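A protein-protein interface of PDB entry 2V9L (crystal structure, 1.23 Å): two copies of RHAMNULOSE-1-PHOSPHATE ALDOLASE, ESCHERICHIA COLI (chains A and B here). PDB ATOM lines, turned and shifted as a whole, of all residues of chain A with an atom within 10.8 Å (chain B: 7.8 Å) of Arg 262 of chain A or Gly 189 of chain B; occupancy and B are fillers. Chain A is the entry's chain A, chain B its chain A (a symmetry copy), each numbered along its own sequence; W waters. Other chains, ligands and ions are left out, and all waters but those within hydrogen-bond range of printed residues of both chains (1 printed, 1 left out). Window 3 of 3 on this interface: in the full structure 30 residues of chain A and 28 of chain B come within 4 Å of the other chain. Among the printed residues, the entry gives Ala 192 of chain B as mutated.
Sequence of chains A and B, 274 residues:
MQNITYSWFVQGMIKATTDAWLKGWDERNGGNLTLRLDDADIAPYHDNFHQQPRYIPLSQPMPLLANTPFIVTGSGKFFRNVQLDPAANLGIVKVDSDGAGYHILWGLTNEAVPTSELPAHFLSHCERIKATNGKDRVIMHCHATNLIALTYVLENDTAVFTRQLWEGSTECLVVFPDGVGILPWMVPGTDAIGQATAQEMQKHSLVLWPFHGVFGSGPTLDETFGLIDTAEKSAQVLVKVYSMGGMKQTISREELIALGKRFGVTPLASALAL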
ATOM      1  N   THR A 170      16.571  24.223  27.098  1.00  0.00           N
ATOM      2  CA  THR A 170      16.015  25.342  26.334  1.00  0.00           C
ATOM      3  C   THR A 170      14.528  25.263  26.154  1.00  0.00           C
ATOM      4  O   THR A 170      13.818  26.291  26.252  1.00  0.00           O
ATOM      5  CB  THR A 170      16.725  25.403  24.969  1.00  0.00           C
ATOM      6  OG1 THR A 170      18.055  25.893  25.187  1.00  0.00           O
ATOM      7  CG2 THR A 170      16.046  26.370  23.994  1.00  0.00           C
ATOM      8  N   GLU A 171      13.964  24.078  25.917  1.00  0.00           N
ATOM      9  CA  GLU A 171      12.532  23.952  25.745  1.00  0.00           C
ATOM     10  C   GLU A 171      11.655  24.354  26.913  1.00  0.00           C
ATOM     11  O   GLU A 171      10.463  24.561  26.729  1.00  0.00           O
ATOM     12  CB  GLU A 171      12.198  22.466  25.421  1.00  0.00           C
ATOM     13  CG  GLU A 171      12.515  21.556  26.580  1.00  0.00           C
ATOM     14  CD  GLU A 171      12.845  20.140  26.266  1.00  0.00           C
ATOM     15  OE1 GLU A 171      12.640  19.642  25.132  1.00  0.00           O
ATOM     16  OE2 GLU A 171      13.278  19.481  27.264  1.00  0.00           O
ATOM     17  N   LEU A 173      11.011  26.922  28.933  1.00  0.00           N
ATOM     18  CA  LEU A 173      10.173  28.139  28.931  1.00  0.00           C
ATOM     19  C   LEU A 173       9.015  27.980  27.991  1.00  0.00           C
ATOM     20  O   LEU A 173       7.923  28.518  28.180  1.00  0.00           O
ATOM     21  CB  LEU A 173      11.068  29.329  28.587  1.00  0.00           C
ATOM     22  CG  LEU A 173      10.328  30.669  28.442  1.00  0.00           C
ATOM     23  CD1 LEU A 173      11.261  31.722  28.937  1.00  0.00           C
ATOM     24  CD2 LEU A 173       9.927  30.958  27.044  1.00  0.00           C
ATOM     25  N   VAL A 174       9.204  27.270  26.861  1.00  0.00           N
ATOM     26  CA  VAL A 174       8.157  27.068  25.857  1.00  0.00           C
ATOM     27  C   VAL A 174       7.125  26.067  26.338  1.00  0.00           C
ATOM     28  O   VAL A 174       5.936  26.222  26.081  1.00  0.00           O
ATOM     29  CB  VAL A 174       8.782  26.675  24.507  1.00  0.00           C
ATOM     30  CG1 VAL A 174       7.693  26.475  23.464  1.00  0.00           C
ATOM     31  CG2 VAL A 174       9.784  27.735  24.098  1.00  0.00           C
ATOM     32  N   PRO A 177       5.678  28.071  30.180  1.00  0.00           N
ATOM     33  CA  PRO A 177       5.935  29.510  30.314  1.00  0.00           C
ATOM     34  C   PRO A 177       5.322  30.092  31.591  1.00  0.00           C
ATOM     35  O   PRO A 177       5.833  31.089  32.107  1.00  0.00           O
ATOM     36  CB  PRO A 177       5.322  30.108  29.036  1.00  0.00           C
ATOM     37  CG  PRO A 177       4.282  29.128  28.652  1.00  0.00           C
ATOM     38  CD  PRO A 177       4.923  27.775  28.929  1.00  0.00           C
ATOM     39  N   GLU A 255      18.065  35.878  26.291  1.00  0.00           N
ATOM     40  CA  GLU A 255      17.781  34.701  25.475  1.00  0.00           C
ATOM     41  C   GLU A 255      16.402  34.133  25.805  1.00  0.00           C
ATOM     42  O   GLU A 255      15.673  33.761  24.904  1.00  0.00           O
ATOM     43  CB  GLU A 255      18.888  33.674  25.735  1.00  0.00           C
ATOM     44  CG  GLU A 255      20.222  34.123  25.125  1.00  0.00           C
ATOM     45  CD  GLU A 255      21.442  33.289  25.539  1.00  0.00           C
ATOM     46  OE1 GLU A 255      22.488  33.390  24.799  1.00  0.00           O
ATOM     47  OE2 GLU A 255      21.385  32.603  26.587  1.00  0.00           O
ATOM     48  N   LEU A 256      16.056  34.075  27.107  1.00  0.00           N
ATOM     49  CA  LEU A 256      14.713  33.608  27.446  1.00  0.00           C
ATOM     50  C   LEU A 256      13.646  34.492  26.836  1.00  0.00           C
ATOM     51  O   LEU A 256      12.609  34.035  26.350  1.00  0.00           O
ATOM     52  CB  LEU A 256      14.511  33.555  28.992  1.00  0.00           C
ATOM     53  CG  LEU A 256      15.418  32.516  29.666  1.00  0.00           C
ATOM     54  CD1 LEU A 256      15.506  32.799  31.146  1.00  0.00           C
ATOM     55  CD2 LEU A 256      14.903  31.123  29.369  1.00  0.00           C
ATOM     56  N   ILE A 257      13.876  35.837  26.847  1.00  0.00           N
ATOM     57  CA  ILE A 257      12.921  36.751  26.259  1.00  0.00           C
ATOM     58  C   ILE A 257      12.774  36.490  24.753  1.00  0.00           C
ATOM     59  O   ILE A 257      11.639  36.389  24.230  1.00  0.00           O
ATOM     60  CB  ILE A 257      13.313  38.213  26.572  1.00  0.00           C
ATOM     61  CG1 ILE A 257      13.093  38.593  28.019  1.00  0.00           C
ATOM     62  CG2 ILE A 257      12.583  39.229  25.650  1.00  0.00           C
ATOM     63  CD1 ILE A 257      13.770  39.907  28.434  1.00  0.00           C
ATOM     64  N   ALA A 258      13.919  36.314  24.063  1.00  0.00           N
ATOM     65  CA  ALA A 258      13.837  36.030  22.622  1.00  0.00           C
ATOM     66  C   ALA A 258      13.116  34.730  22.326  1.00  0.00           C
ATOM     67  O   ALA A 258      12.346  34.581  21.367  1.00  0.00           O
ATOM     68  CB  ALA A 258      15.253  36.019  22.023  1.00  0.00           C
ATOM     69  N   LEU A 259      13.384  33.718  23.159  1.00  0.00           N
ATOM     70  CA  LEU A 259      12.736  32.430  23.016  1.00  0.00           C
ATOM     71  C   LEU A 259      11.219  32.520  23.131  1.00  0.00           C
ATOM     72  O   LEU A 259      10.436  32.007  22.328  1.00  0.00           O
ATOM     73  CB  LEU A 259      13.317  31.531  24.131  1.00  0.00           C
ATOM     74  CG  LEU A 259      12.895  30.077  24.067  1.00  0.00           C
ATOM     75  CD1 LEU A 259      13.398  29.339  22.844  1.00  0.00           C
ATOM     76  CD2 LEU A 259      13.528  29.379  25.289  1.00  0.00           C
ATOM     77  N   GLY A 260      10.806  33.261  24.191  1.00  0.00           N
ATOM     78  CA  GLY A 260       9.371  33.432  24.351  1.00  0.00           C
ATOM     79  C   GLY A 260       8.689  34.158  23.220  1.00  0.00           C
ATOM     80  O   GLY A 260       7.592  33.808  22.768  1.00  0.00           O
ATOM     81  N   LYS A 261       9.356  35.191  22.708  1.00  0.00           N
ATOM     82  CA  LYS A 261       8.817  35.912  21.552  1.00  0.00           C
ATOM     83  C   LYS A 261       8.659  35.040  20.326  1.00  0.00           C
ATOM     84  O   LYS A 261       7.657  35.026  19.640  1.00  0.00           O
ATOM     85  CB  LYS A 261       9.768  37.070  21.200  1.00  0.00           C
ATOM     86  CG  LYS A 261       9.839  38.158  22.264  1.00  0.00           C
ATOM     87  CD  LYS A 261      10.407  39.478  21.837  1.00  0.00           C
ATOM     88  CE  LYS A 261      10.391  40.487  22.973  1.00  0.00           C
ATOM     89  NZ  LYS A 261      11.494  41.514  22.906  1.00  0.00           N
ATOM     90  N   ARG A 262       9.695  34.229  20.050  1.00  0.00           N
ATOM     91  CA  ARG A 262       9.621  33.338  18.888  1.00  0.00           C
ATOM     92  C   ARG A 262       8.513  32.323  18.987  1.00  0.00           C
ATOM     93  O   ARG A 262       7.942  31.942  17.917  1.00  0.00           O
ATOM     94  CB  ARG A 262      10.914  32.562  18.541  1.00  0.00           C
ATOM     95  CG  ARG A 262      10.921  31.720  17.263  1.00  0.00           C
ATOM     96  CD  ARG A 262      11.216  30.254  17.279  1.00  0.00           C
ATOM     97  NE  ARG A 262      11.138  29.278  16.148  1.00  0.00           N
ATOM     98  CZ  ARG A 262      10.041  28.942  15.552  1.00  0.00           C
ATOM     99  NH1 ARG A 262       8.874  29.525  15.945  1.00  0.00           N
ATOM    100  NH2 ARG A 262       9.999  28.058  14.571  1.00  0.00           N
ATOM    101  N   PHE A 263       8.294  31.827  20.193  1.00  0.00           N
ATOM    102  CA  PHE A 263       7.299  30.780  20.313  1.00  0.00           C
ATOM    103  C   PHE A 263       5.972  31.331  20.762  1.00  0.00           C
ATOM    104  O   PHE A 263       5.020  30.558  21.034  1.00  0.00           O
ATOM    105  CB  PHE A 263       7.816  29.687  21.253  1.00  0.00           C
ATOM    106  CG  PHE A 263       8.859  28.865  20.519  1.00  0.00           C
ATOM    107  CD1 PHE A 263      10.194  29.100  20.696  1.00  0.00           C
ATOM    108  CD2 PHE A 263       8.464  27.890  19.630  1.00  0.00           C
ATOM    109  CE1 PHE A 263      11.073  28.331  19.948  1.00  0.00           C
ATOM    110  CE2 PHE A 263       9.363  27.130  18.905  1.00  0.00           C
ATOM    111  CZ  PHE A 263      10.695  27.349  19.063  1.00  0.00           C
ATOM    112  N   GLY A 264       5.801  32.661  20.855  1.00  0.00           N
ATOM    113  CA  GLY A 264       4.515  33.247  21.178  1.00  0.00           C
ATOM    114  C   GLY A 264       4.007  32.922  22.579  1.00  0.00           C
ATOM    115  O   GLY A 264       2.779  32.757  22.701  1.00  0.00           O
ATOM    116  N   VAL A 265       4.901  32.842  23.557  1.00  0.00           N
ATOM    117  CA  VAL A 265       4.468  32.618  24.931  1.00  0.00           C
ATOM    118  C   VAL A 265       4.945  33.798  25.788  1.00  0.00           C
ATOM    119  O   VAL A 265       5.943  34.433  25.489  1.00  0.00           O
ATOM    120  CB  VAL A 265       4.973  31.288  25.516  1.00  0.00           C
ATOM    121  CG1 VAL A 265       4.425  30.116  24.769  1.00  0.00           C
ATOM    122  CG2 VAL A 265       6.490  31.231  25.504  1.00  0.00           C
ATOM    123  N   THR A 266       4.165  34.014  26.841  1.00  0.00           N
ATOM    124  CA  THR A 266       4.465  35.056  27.799  1.00  0.00           C
ATOM    125  C   THR A 266       5.101  34.419  29.054  1.00  0.00           C
ATOM    126  O   THR A 266       4.419  33.738  29.859  1.00  0.00           O
ATOM    127  CB  THR A 266       3.199  35.812  28.235  1.00  0.00           C
ATOM    128  OG1 THR A 266       2.616  36.406  27.074  1.00  0.00           O
ATOM    129  CG2 THR A 266       3.543  36.875  29.263  1.00  0.00           C
ATOM    130  N   PRO A 267       6.389  34.616  29.252  1.00  0.00           N
ATOM    131  CA  PRO A 267       7.001  33.965  30.388  1.00  0.00           C
ATOM    132  C   PRO A 267       6.613  34.601  31.705  1.00  0.00           C
ATOM    133  O   PRO A 267       6.428  35.805  31.757  1.00  0.00           O
ATOM    134  CB  PRO A 267       8.494  34.217  30.154  1.00  0.00           C
ATOM    135  CG  PRO A 267       8.645  34.613  28.730  1.00  0.00           C
ATOM    136  CD  PRO A 267       7.372  35.363  28.448  1.00  0.00           C
ATOM    137  N   THR B 115       9.363  17.752  11.279  1.00  0.00           N
ATOM    138  CA  THR B 115       9.979  18.475  12.342  1.00  0.00           C
ATOM    139  C   THR B 115      10.206  19.961  12.047  1.00  0.00           C
ATOM    140  O   THR B 115      10.584  20.351  10.948  1.00  0.00           O
ATOM    141  CB  THR B 115      11.350  17.831  12.692  1.00  0.00           C
ATOM    142  OG1 THR B 115      12.036  18.659  13.632  1.00  0.00           O
ATOM    143  CG2 THR B 115      12.319  17.753  11.518  1.00  0.00           C
ATOM    144  N   SER B 116       9.984  20.796  13.061  1.00  0.00           N
ATOM    145  CA  SER B 116      10.250  22.221  13.011  1.00  0.00           C
ATOM    146  C   SER B 116      11.731  22.527  12.833  1.00  0.00           C
ATOM    147  O   SER B 116      12.037  23.672  12.520  1.00  0.00           O
ATOM    148  CB  SER B 116       9.773  22.946  14.276  1.00  0.00           C
ATOM    149  OG  SER B 116      10.616  22.818  15.373  1.00  0.00           O
ATOM    150  N   GLU B 117      12.624  21.565  13.016  1.00  0.00           N
ATOM    151  CA  GLU B 117      14.051  21.729  12.794  1.00  0.00           C
ATOM    152  C   GLU B 117      14.421  21.269  11.383  1.00  0.00           C
ATOM    153  O   GLU B 117      15.606  21.021  11.105  1.00  0.00           O
ATOM    154  CB  GLU B 117      14.877  21.008  13.830  1.00  0.00           C
ATOM    155  CG  GLU B 117      14.771  21.607  15.203  1.00  0.00           C
ATOM    156  CD  GLU B 117      15.267  23.015  15.381  1.00  0.00           C
ATOM    157  OE1 GLU B 117      15.115  23.497  16.557  1.00  0.00           O
ATOM    158  OE2 GLU B 117      15.800  23.656  14.512  1.00  0.00           O
ATOM    159  N   LEU B 118      13.447  21.224  10.491  1.00  0.00           N
ATOM    160  CA  LEU B 118      13.781  20.833   9.115  1.00  0.00           C
ATOM    161  C   LEU B 118      14.858  21.688   8.502  1.00  0.00           C
ATOM    162  O   LEU B 118      15.710  21.124   7.765  1.00  0.00           O
ATOM    163  CB  LEU B 118      12.512  20.782   8.245  1.00  0.00           C
ATOM    164  CG  LEU B 118      12.648  19.924   6.968  1.00  0.00           C
ATOM    165  CD1 LEU B 118      12.783  18.445   7.316  1.00  0.00           C
ATOM    166  CD2 LEU B 118      11.458  20.177   6.052  1.00  0.00           C
ATOM    167  N   PRO B 119      14.924  22.994   8.702  1.00  0.00           N
ATOM    168  CA  PRO B 119      16.071  23.739   8.124  1.00  0.00           C
ATOM    169  C   PRO B 119      17.406  23.176   8.587  1.00  0.00           C
ATOM    170  O   PRO B 119      18.291  22.881   7.790  1.00  0.00           O
ATOM    171  CB  PRO B 119      15.829  25.199   8.556  1.00  0.00           C
ATOM    172  CG  PRO B 119      14.342  25.285   8.752  1.00  0.00           C
ATOM    173  CD  PRO B 119      13.996  23.914   9.352  1.00  0.00           C
ATOM    174  N   ALA B 120      17.577  23.032   9.921  1.00  0.00           N
ATOM    175  CA  ALA B 120      18.830  22.468  10.430  1.00  0.00           C
ATOM    176  C   ALA B 120      19.103  21.101   9.815  1.00  0.00           C
ATOM    177  O   ALA B 120      20.234  20.809   9.453  1.00  0.00           O
ATOM    178  CB  ALA B 120      18.793  22.365  11.953  1.00  0.00           C
ATOM    179  N   MET B 186      21.362  29.761  20.453  1.00  0.00           N
ATOM    180  CA  MET B 186      20.522  30.421  19.464  1.00  0.00           C
ATOM    181  C   MET B 186      19.084  29.971  19.601  1.00  0.00           C
ATOM    182  O   MET B 186      18.792  28.898  20.118  1.00  0.00           O
ATOM    183  CB  MET B 186      21.005  30.114  18.043  1.00  0.00           C
ATOM    184  CG  MET B 186      22.395  30.634  17.748  1.00  0.00           C
ATOM    185  SD  MET B 186      23.041  30.181  16.141  1.00  0.00           S
ATOM    186  CE  MET B 186      21.963  31.098  15.038  1.00  0.00           C
ATOM    187  N   VAL B 187      18.123  30.799  19.182  1.00  0.00           N
ATOM    188  CA  VAL B 187      16.732  30.420  19.196  1.00  0.00           C
ATOM    189  C   VAL B 187      16.492  29.249  18.240  1.00  0.00           C
ATOM    190  O   VAL B 187      16.870  29.294  17.078  1.00  0.00           O
ATOM    191  CB  VAL B 187      15.890  31.649  18.770  1.00  0.00           C
ATOM    192  CG1 VAL B 187      14.423  31.267  18.652  1.00  0.00           C
ATOM    193  CG2 VAL B 187      16.085  32.842  19.703  1.00  0.00           C
ATOM    194  N   PRO B 188      15.894  28.185  18.765  1.00  0.00           N
ATOM    195  CA  PRO B 188      15.667  26.967  17.927  1.00  0.00           C
ATOM    196  C   PRO B 188      14.561  27.176  16.889  1.00  0.00           C
ATOM    197  O   PRO B 188      13.724  28.085  17.012  1.00  0.00           O
ATOM    198  CB  PRO B 188      15.337  25.907  18.953  1.00  0.00           C
ATOM    199  CG  PRO B 188      15.130  26.524  20.232  1.00  0.00           C
ATOM    200  CD  PRO B 188      15.452  27.974  20.177  1.00  0.00           C
ATOM    201  N   GLY B 189      14.539  26.303  15.910  1.00  0.00           N
ATOM    202  CA  GLY B 189      13.500  26.234  14.940  1.00  0.00           C
ATOM    203  C   GLY B 189      13.548  27.337  13.902  1.00  0.00           C
ATOM    204  O   GLY B 189      12.584  27.690  13.273  1.00  0.00           O
ATOM    205  N   THR B 190      14.708  27.931  13.723  1.00  0.00           N
ATOM    206  CA  THR B 190      14.906  29.085  12.820  1.00  0.00           C
ATOM    207  C   THR B 190      15.820  28.696  11.667  1.00  0.00           C
ATOM    208  O   THR B 190      16.598  27.751  11.753  1.00  0.00           O
ATOM    209  CB  THR B 190      15.515  30.279  13.579  1.00  0.00           C
ATOM    210  OG1 THR B 190      16.834  29.882  14.043  1.00  0.00           O
ATOM    211  CG2 THR B 190      14.671  30.761  14.739  1.00  0.00           C
ATOM    212  N   ASP B 191      15.861  29.414  10.504  1.00  0.00           N
ATOM    213  CA  ASP B 191      16.906  29.077   9.515  1.00  0.00           C
ATOM    214  C   ASP B 191      18.247  29.645  10.011  1.00  0.00           C
ATOM    215  O   ASP B 191      19.232  29.135   9.514  1.00  0.00           O
ATOM    216  CB  ASP B 191      16.816  29.544   8.045  1.00  0.00           C
ATOM    217  CG  ASP B 191      15.613  28.956   7.321  1.00  0.00           C
ATOM    218  OD1 ASP B 191      14.512  29.430   7.598  1.00  0.00           O
ATOM    219  OD2 ASP B 191      15.836  28.022   6.510  1.00  0.00           O
ATOM    220  N   ALA B 192      18.237  30.672  10.899  1.00  0.00           N
ATOM    221  CA  ALA B 192      19.551  31.017  11.413  1.00  0.00           C
ATOM    222  C   ALA B 192      20.238  29.855  12.103  1.00  0.00           C
ATOM    223  O   ALA B 192      21.419  29.564  11.832  1.00  0.00           O
ATOM    224  CB  ALA B 192      19.467  32.211  12.367  1.00  0.00           C
ATOM    225  N   ILE B 193      19.545  29.181  13.040  1.00  0.00           N
ATOM    226  CA  ILE B 193      20.222  28.092  13.732  1.00  0.00           C
ATOM    227  C   ILE B 193      20.456  26.955  12.802  1.00  0.00           C
ATOM    228  O   ILE B 193      21.454  26.227  12.905  1.00  0.00           O
ATOM    229  CB  ILE B 193      19.441  27.663  15.016  1.00  0.00           C
ATOM    230  CG1 ILE B 193      20.353  26.958  16.004  1.00  0.00           C
ATOM    231  CG2 ILE B 193      18.237  26.815  14.680  1.00  0.00           C
ATOM    232  CD1 ILE B 193      19.666  26.633  17.335  1.00  0.00           C
ATOM    233  N   GLY B 194      19.547  26.782  11.814  1.00  0.00           N
ATOM    234  CA  GLY B 194      19.780  25.719  10.860  1.00  0.00           C
ATOM    235  C   GLY B 194      21.016  25.911   9.986  1.00  0.00           C
ATOM    236  O   GLY B 194      21.822  25.005   9.766  1.00  0.00           O
ATOM    237  N   TRP B 209      24.568  22.379  20.622  1.00  0.00           N
ATOM    238  CA  TRP B 209      23.655  23.500  20.860  1.00  0.00           C
ATOM    239  C   TRP B 209      23.697  23.707  22.375  1.00  0.00           C
ATOM    240  O   TRP B 209      23.073  22.889  23.112  1.00  0.00           O
ATOM    241  CB  TRP B 209      22.258  23.187  20.352  1.00  0.00           C
ATOM    242  CG  TRP B 209      22.078  23.260  18.866  1.00  0.00           C
ATOM    243  CD1 TRP B 209      23.027  23.394  17.906  1.00  0.00           C
ATOM    244  CD2 TRP B 209      20.834  23.194  18.187  1.00  0.00           C
ATOM    245  NE1 TRP B 209      22.419  23.428  16.656  1.00  0.00           N
ATOM    246  CE2 TRP B 209      21.084  23.331  16.815  1.00  0.00           C
ATOM    247  CE3 TRP B 209      19.514  23.074  18.643  1.00  0.00           C
ATOM    248  CZ2 TRP B 209      20.056  23.347  15.866  1.00  0.00           C
ATOM    249  CZ3 TRP B 209      18.485  23.081  17.682  1.00  0.00           C
ATOM    250  CH2 TRP B 209      18.771  23.223  16.308  1.00  0.00           C
ATOM    251  N   HIS B 212      20.935  22.820  25.288  1.00  0.00           N
ATOM    252  CA  HIS B 212      19.907  22.276  24.410  1.00  0.00           C
ATOM    253  C   HIS B 212      20.238  20.840  24.018  1.00  0.00           C
ATOM    254  O   HIS B 212      19.469  19.917  24.327  1.00  0.00           O
ATOM    255  CB  HIS B 212      19.636  23.238  23.233  1.00  0.00           C
ATOM    256  CG  HIS B 212      18.482  22.786  22.377  1.00  0.00           C
ATOM    257  ND1 HIS B 212      17.766  23.662  21.566  1.00  0.00           N
ATOM    258  CD2 HIS B 212      17.872  21.609  22.099  1.00  0.00           C
ATOM    259  CE1 HIS B 212      16.853  22.986  20.889  1.00  0.00           C
ATOM    260  NE2 HIS B 212      16.861  21.663  21.202  1.00  0.00           N
HETATM  261  O   HOH W   1      10.204  25.946  15.869  1.00  0.00           O
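NH2 of Arg 262 of chain A is in hydrogen-bond range of O of Gly 189 of chain B, 2.9 Å away. The guanidinium group of Arg 262 of chain A sits at hydrogen-bond distance from the backbone carbonyl oxygen of Pro 188 of chain B (3.0 Å).
No position is printed for both chains.
Water W1 lies within hydrogen-bond range of the guanidinium group (NH2) of Arg 262 of chain A (2.5 Å) and the side-chain hydroxyl (OG) of Ser 116 of chain B (3.2 Å).
Of the 18 printed residues of chain A, 4 touch a printed residue of chain B. Printed residues of chain B that touch a printed residue of chain A: Val 187, Pro 188, Gly 189 and His 212.
Printed residues of chain B within 4 Å of Thr 170 of chain A: Pro 188 and His 212. Printed residues of chain B within 4 Å of Arg 262 of chain A: Val 187, Pro 188 and Gly 189. Printed residues of chain B within 4 Å of Phe 263 of chain A: Pro 188 (3.7 Å). Printed residues of chain A within 4 Å of Val 187 of chain B: Arg 262. Printed residues of chain A within 4 Å of Gly 189 of chain B: Arg 262 (2.9 Å). Of the printed residues of chain A, His 212 of chain B touches Thr 170. The nearest printed residue of chain B that does not touch Arg 262 of chain A is Thr 190 of chain B (4.1 Å). The nearest printed residue of chain A that does not touch Gly 189 of chain B is Phe 263 of chain A (5.1 Å). The nearest printed residue of chain B that does not touch Phe 263 of chain A is Val 187 of chain B (4.6 Å).
Among the printed residues, pairs that only touch across the chains: Thr 170 of chain A with Pro 188 of chain B (3.9 Å), Thr 170 of chain A with His 212 of chain B (3.7 Å), Leu 259 of chain A with Pro 188 of chain B (3.6 Å), Arg 262 of chain A with Val 187 of chain B (3.6 Å) and Phe 263 of chain A with Pro 188 of chain B (3.7 Å).
O of Val 187 of chain B lies within hydrogen-bond range of OG1 of Thr 190 of chain B (3.1 Å). OE1 of Glu 117 of chain B is in hydrogen-bond range of N of Gly 189 of chain B, 2.9 Å away.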
